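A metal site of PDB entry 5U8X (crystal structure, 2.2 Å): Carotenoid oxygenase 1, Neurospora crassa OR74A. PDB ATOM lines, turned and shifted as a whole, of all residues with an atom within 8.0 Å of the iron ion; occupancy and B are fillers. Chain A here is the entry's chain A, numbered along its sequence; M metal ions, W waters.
A ring nitrogen (ND1) of His 510 lies within hydrogen-bond range of the side-chain carboxylate (OE2) of Glu 453, at 2.8 Å. A ring nitrogen (ND1) of His 248 lies within hydrogen-bond range of the side-chain carboxylate (OE2) of Glu 165 (2.7 Å). O of Thr 151 is in hydrogen-bond range of N of His 510. A ring nitrogen (ND1) of His 313 sits at hydrogen-bond distance from the side-chain carboxylate of Glu 383 (2.7 Å).
Four residues have an atom within 4 Å of the iron ion: His 197, His 248, His 313 and His 510.
A ring nitrogen (NE2) of His 248 is bound to the iron ion, 2.0 Å away. NE2 of His 510 binds the iron ion. The iron ion is bound by NE2 of His 313, 2.2 Å away. The iron ion is bound by NE2 of His 197. The iron ion has four donor atoms within binding distance.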
ATOM      1  N   PHE A  91      31.191   1.128  -3.810  1.00  0.00           N
ATOM      2  CA  PHE A  91      30.064   2.038  -3.674  1.00  0.00           C
ATOM      3  C   PHE A  91      29.422   2.030  -2.287  1.00  0.00           C
ATOM      4  O   PHE A  91      28.527   2.834  -2.035  1.00  0.00           O
ATOM      5  CB  PHE A  91      28.949   1.682  -4.677  1.00  0.00           C
ATOM      6  CG  PHE A  91      29.148   2.121  -6.107  1.00  0.00           C
ATOM      7  CD1 PHE A  91      30.182   2.964  -6.489  1.00  0.00           C
ATOM      8  CD2 PHE A  91      28.293   1.646  -7.098  1.00  0.00           C
ATOM      9  CE1 PHE A  91      30.346   3.355  -7.806  1.00  0.00           C
ATOM     10  CE2 PHE A  91      28.458   2.026  -8.425  1.00  0.00           C
ATOM     11  CZ  PHE A  91      29.484   2.885  -8.774  1.00  0.00           C
ATOM     12  N   THR A 151      28.687   9.837  -2.866  1.00  0.00           N
ATOM     13  CA  THR A 151      28.671   9.870  -4.321  1.00  0.00           C
ATOM     14  C   THR A 151      29.045  11.249  -4.857  1.00  0.00           C
ATOM     15  O   THR A 151      29.836  11.346  -5.784  1.00  0.00           O
ATOM     16  CB  THR A 151      27.310   9.429  -4.879  1.00  0.00           C
ATOM     17  OG1 THR A 151      27.029   8.128  -4.364  1.00  0.00           O
ATOM     18  CG2 THR A 151      27.300   9.390  -6.391  1.00  0.00           C
ATOM     19  N   ASN A 152      28.437  12.298  -4.308  1.00  0.00           N
ATOM     20  CA  ASN A 152      28.689  13.638  -4.776  1.00  0.00           C
ATOM     21  C   ASN A 152      28.590  14.613  -3.602  1.00  0.00           C
ATOM     22  O   ASN A 152      28.031  14.282  -2.564  1.00  0.00           O
ATOM     23  CB  ASN A 152      27.741  14.015  -5.918  1.00  0.00           C
ATOM     24  CG  ASN A 152      28.228  15.166  -6.772  1.00  0.00           C
ATOM     25  OD1 ASN A 152      29.294  15.714  -6.542  1.00  0.00           O
ATOM     26  ND2 ASN A 152      27.439  15.542  -7.766  1.00  0.00           N
ATOM     27  N   GLU A 165      22.047   8.426  -3.796  1.00  0.00           N
ATOM     28  CA  GLU A 165      20.801   8.406  -4.553  1.00  0.00           C
ATOM     29  C   GLU A 165      19.714   7.572  -3.868  1.00  0.00           C
ATOM     30  O   GLU A 165      18.572   7.604  -4.327  1.00  0.00           O
ATOM     31  CB  GLU A 165      21.051   7.921  -5.979  1.00  0.00           C
ATOM     32  CG  GLU A 165      21.510   6.476  -6.109  1.00  0.00           C
ATOM     33  CD  GLU A 165      22.197   6.161  -7.427  1.00  0.00           C
ATOM     34  OE1 GLU A 165      21.765   5.203  -8.105  1.00  0.00           O
ATOM     35  OE2 GLU A 165      23.148   6.888  -7.787  1.00  0.00           O
ATOM     36  N   ALA A 196      22.207  11.955  -6.937  1.00  0.00           N
ATOM     37  CA  ALA A 196      23.574  12.397  -6.720  1.00  0.00           C
ATOM     38  C   ALA A 196      24.000  13.390  -7.799  1.00  0.00           C
ATOM     39  O   ALA A 196      25.096  13.942  -7.728  1.00  0.00           O
ATOM     40  CB  ALA A 196      24.488  11.209  -6.696  1.00  0.00           C
ATOM     41  N   HIS A 197      23.151  13.620  -8.817  1.00  0.00           N
ATOM     42  CA  HIS A 197      23.516  14.455  -9.940  1.00  0.00           C
ATOM     43  C   HIS A 197      22.452  15.527 -10.196  1.00  0.00           C
ATOM     44  O   HIS A 197      21.869  15.577 -11.271  1.00  0.00           O
ATOM     45  CB  HIS A 197      23.768  13.580 -11.167  1.00  0.00           C
ATOM     46  CG  HIS A 197      25.041  12.816 -11.042  1.00  0.00           C
ATOM     47  ND1 HIS A 197      26.243  13.482 -11.118  1.00  0.00           N
ATOM     48  CD2 HIS A 197      25.321  11.525 -10.823  1.00  0.00           C
ATOM     49  CE1 HIS A 197      27.218  12.606 -10.952  1.00  0.00           C
ATOM     50  NE2 HIS A 197      26.675  11.408 -10.775  1.00  0.00           N
ATOM     51  N   HIS A 248      20.766   6.886 -12.500  1.00  0.00           N
ATOM     52  CA  HIS A 248      21.897   7.453 -11.785  1.00  0.00           C
ATOM     53  C   HIS A 248      22.051   8.945 -12.070  1.00  0.00           C
ATOM     54  O   HIS A 248      22.316   9.738 -11.165  1.00  0.00           O
ATOM     55  CB  HIS A 248      23.203   6.738 -12.166  1.00  0.00           C
ATOM     56  CG  HIS A 248      24.398   7.307 -11.472  1.00  0.00           C
ATOM     57  ND1 HIS A 248      24.561   7.234 -10.104  1.00  0.00           N
ATOM     58  CD2 HIS A 248      25.459   7.963 -11.934  1.00  0.00           C
ATOM     59  CE1 HIS A 248      25.703   7.830  -9.768  1.00  0.00           C
ATOM     60  NE2 HIS A 248      26.263   8.280 -10.875  1.00  0.00           N
ATOM     61  N   ASP A 249      21.905   9.308 -13.342  1.00  0.00           N
ATOM     62  CA  ASP A 249      22.103  10.674 -13.786  1.00  0.00           C
ATOM     63  C   ASP A 249      20.878  11.092 -14.585  1.00  0.00           C
ATOM     64  O   ASP A 249      20.057  10.253 -14.934  1.00  0.00           O
ATOM     65  CB  ASP A 249      23.412  10.778 -14.580  1.00  0.00           C
ATOM     66  CG  ASP A 249      24.009  12.173 -14.672  1.00  0.00           C
ATOM     67  OD1 ASP A 249      23.292  13.141 -14.352  1.00  0.00           O
ATOM     68  OD2 ASP A 249      25.199  12.254 -15.041  1.00  0.00           O
ATOM     69  N   GLY A 312      25.790   5.984 -18.958  1.00  0.00           N
ATOM     70  CA  GLY A 312      26.822   6.579 -18.117  1.00  0.00           C
ATOM     71  C   GLY A 312      26.462   8.017 -17.722  1.00  0.00           C
ATOM     72  O   GLY A 312      25.314   8.425 -17.812  1.00  0.00           O
ATOM     73  N   HIS A 313      27.476   8.776 -17.289  1.00  0.00           N
ATOM     74  CA  HIS A 313      27.268  10.135 -16.818  1.00  0.00           C
ATOM     75  C   HIS A 313      26.926  11.058 -17.980  1.00  0.00           C
ATOM     76  O   HIS A 313      27.470  10.936 -19.072  1.00  0.00           O
ATOM     77  CB  HIS A 313      28.500  10.616 -16.040  1.00  0.00           C
ATOM     78  CG  HIS A 313      28.633   9.955 -14.715  1.00  0.00           C
ATOM     79  ND1 HIS A 313      29.593   9.018 -14.430  1.00  0.00           N
ATOM     80  CD2 HIS A 313      27.891  10.082 -13.620  1.00  0.00           C
ATOM     81  CE1 HIS A 313      29.441   8.604 -13.178  1.00  0.00           C
ATOM     82  NE2 HIS A 313      28.405   9.244 -12.666  1.00  0.00           N
ATOM     83  N   VAL A 314      25.999  11.992 -17.712  1.00  0.00           N
ATOM     84  CA  VAL A 314      25.616  13.017 -18.649  1.00  0.00           C
ATOM     85  C   VAL A 314      26.663  14.131 -18.644  1.00  0.00           C
ATOM     86  O   VAL A 314      27.011  14.639 -17.583  1.00  0.00           O
ATOM     87  CB  VAL A 314      24.227  13.573 -18.305  1.00  0.00           C
ATOM     88  CG1 VAL A 314      23.861  14.764 -19.173  1.00  0.00           C
ATOM     89  CG2 VAL A 314      23.156  12.485 -18.390  1.00  0.00           C
ATOM     90  N   PHE A 337      28.649  -2.125 -14.635  1.00  0.00           N
ATOM     91  CA  PHE A 337      28.631  -2.643 -13.265  1.00  0.00           C
ATOM     92  C   PHE A 337      28.538  -4.173 -13.305  1.00  0.00           C
ATOM     93  O   PHE A 337      27.518  -4.744 -12.920  1.00  0.00           O
ATOM     94  CB  PHE A 337      27.495  -1.996 -12.476  1.00  0.00           C
ATOM     95  CG  PHE A 337      27.540  -0.487 -12.344  1.00  0.00           C
ATOM     96  CD1 PHE A 337      28.684   0.241 -12.652  1.00  0.00           C
ATOM     97  CD2 PHE A 337      26.414   0.212 -11.936  1.00  0.00           C
ATOM     98  CE1 PHE A 337      28.702   1.622 -12.558  1.00  0.00           C
ATOM     99  CE2 PHE A 337      26.438   1.596 -11.824  1.00  0.00           C
ATOM    100  CZ  PHE A 337      27.572   2.296 -12.136  1.00  0.00           C
ATOM    101  N   GLU A 383      34.830   8.444 -19.428  1.00  0.00           N
ATOM    102  CA  GLU A 383      33.777   8.667 -18.442  1.00  0.00           C
ATOM    103  C   GLU A 383      34.035   9.983 -17.709  1.00  0.00           C
ATOM    104  O   GLU A 383      35.001  10.680 -18.017  1.00  0.00           O
ATOM    105  CB  GLU A 383      33.668   7.479 -17.467  1.00  0.00           C
ATOM    106  CG  GLU A 383      32.364   6.689 -17.607  1.00  0.00           C
ATOM    107  CD  GLU A 383      31.091   7.393 -17.130  1.00  0.00           C
ATOM    108  OE1 GLU A 383      31.203   8.474 -16.519  1.00  0.00           O
ATOM    109  OE2 GLU A 383      29.989   6.872 -17.383  1.00  0.00           O
ATOM    110  N   PHE A 384      33.142  10.321 -16.770  1.00  0.00           N
ATOM    111  CA  PHE A 384      33.282  11.459 -15.889  1.00  0.00           C
ATOM    112  C   PHE A 384      33.412  12.751 -16.693  1.00  0.00           C
ATOM    113  O   PHE A 384      34.357  13.510 -16.514  1.00  0.00           O
ATOM    114  CB  PHE A 384      34.441  11.244 -14.902  1.00  0.00           C
ATOM    115  CG  PHE A 384      34.184  10.133 -13.909  1.00  0.00           C
ATOM    116  CD1 PHE A 384      33.242  10.290 -12.899  1.00  0.00           C
ATOM    117  CD2 PHE A 384      34.841   8.912 -14.017  1.00  0.00           C
ATOM    118  CE1 PHE A 384      32.991   9.268 -12.004  1.00  0.00           C
ATOM    119  CE2 PHE A 384      34.579   7.885 -13.128  1.00  0.00           C
ATOM    120  CZ  PHE A 384      33.648   8.060 -12.124  1.00  0.00           C
ATOM    121  N   GLU A 453      37.980  12.205 -11.360  1.00  0.00           N
ATOM    122  CA  GLU A 453      37.157  13.177 -12.068  1.00  0.00           C
ATOM    123  C   GLU A 453      37.758  14.569 -11.885  1.00  0.00           C
ATOM    124  O   GLU A 453      38.152  14.941 -10.790  1.00  0.00           O
ATOM    125  CB  GLU A 453      35.711  13.151 -11.556  1.00  0.00           C
ATOM    126  CG  GLU A 453      34.794  14.149 -12.246  1.00  0.00           C
ATOM    127  CD  GLU A 453      33.489  14.430 -11.523  1.00  0.00           C
ATOM    128  OE1 GLU A 453      33.550  14.945 -10.376  1.00  0.00           O
ATOM    129  OE2 GLU A 453      32.409  14.147 -12.101  1.00  0.00           O
ATOM    130  N   LEU A 509      34.713   9.593  -6.046  1.00  0.00           N
ATOM    131  CA  LEU A 509      33.695   9.808  -7.048  1.00  0.00           C
ATOM    132  C   LEU A 509      33.684  11.293  -7.415  1.00  0.00           C
ATOM    133  O   LEU A 509      34.709  11.813  -7.859  1.00  0.00           O
ATOM    134  CB  LEU A 509      32.366   9.271  -6.500  1.00  0.00           C
ATOM    135  CG  LEU A 509      32.275   7.740  -6.507  1.00  0.00           C
ATOM    136  CD1 LEU A 509      31.121   7.238  -5.661  1.00  0.00           C
ATOM    137  CD2 LEU A 509      32.140   7.224  -7.927  1.00  0.00           C
ATOM    138  N   HIS A 510      32.567  11.986  -7.201  1.00  0.00           N
ATOM    139  CA  HIS A 510      32.370  13.289  -7.801  1.00  0.00           C
ATOM    140  C   HIS A 510      32.900  14.391  -6.887  1.00  0.00           C
ATOM    141  O   HIS A 510      33.071  14.207  -5.688  1.00  0.00           O
ATOM    142  CB  HIS A 510      30.899  13.476  -8.179  1.00  0.00           C
ATOM    143  CG  HIS A 510      30.452  12.473  -9.197  1.00  0.00           C
ATOM    144  ND1 HIS A 510      30.837  12.528 -10.514  1.00  0.00           N
ATOM    145  CD2 HIS A 510      29.670  11.397  -9.073  1.00  0.00           C
ATOM    146  CE1 HIS A 510      30.301  11.498 -11.158  1.00  0.00           C
ATOM    147  NE2 HIS A 510      29.583  10.791 -10.295  1.00  0.00           N
HETATM  148 FE    FE M   1      27.945   9.358 -10.484  1.00  0.00          FE
HETATM  149  O   HOH W   1      28.909   6.698  -9.385  1.00  0.00           O
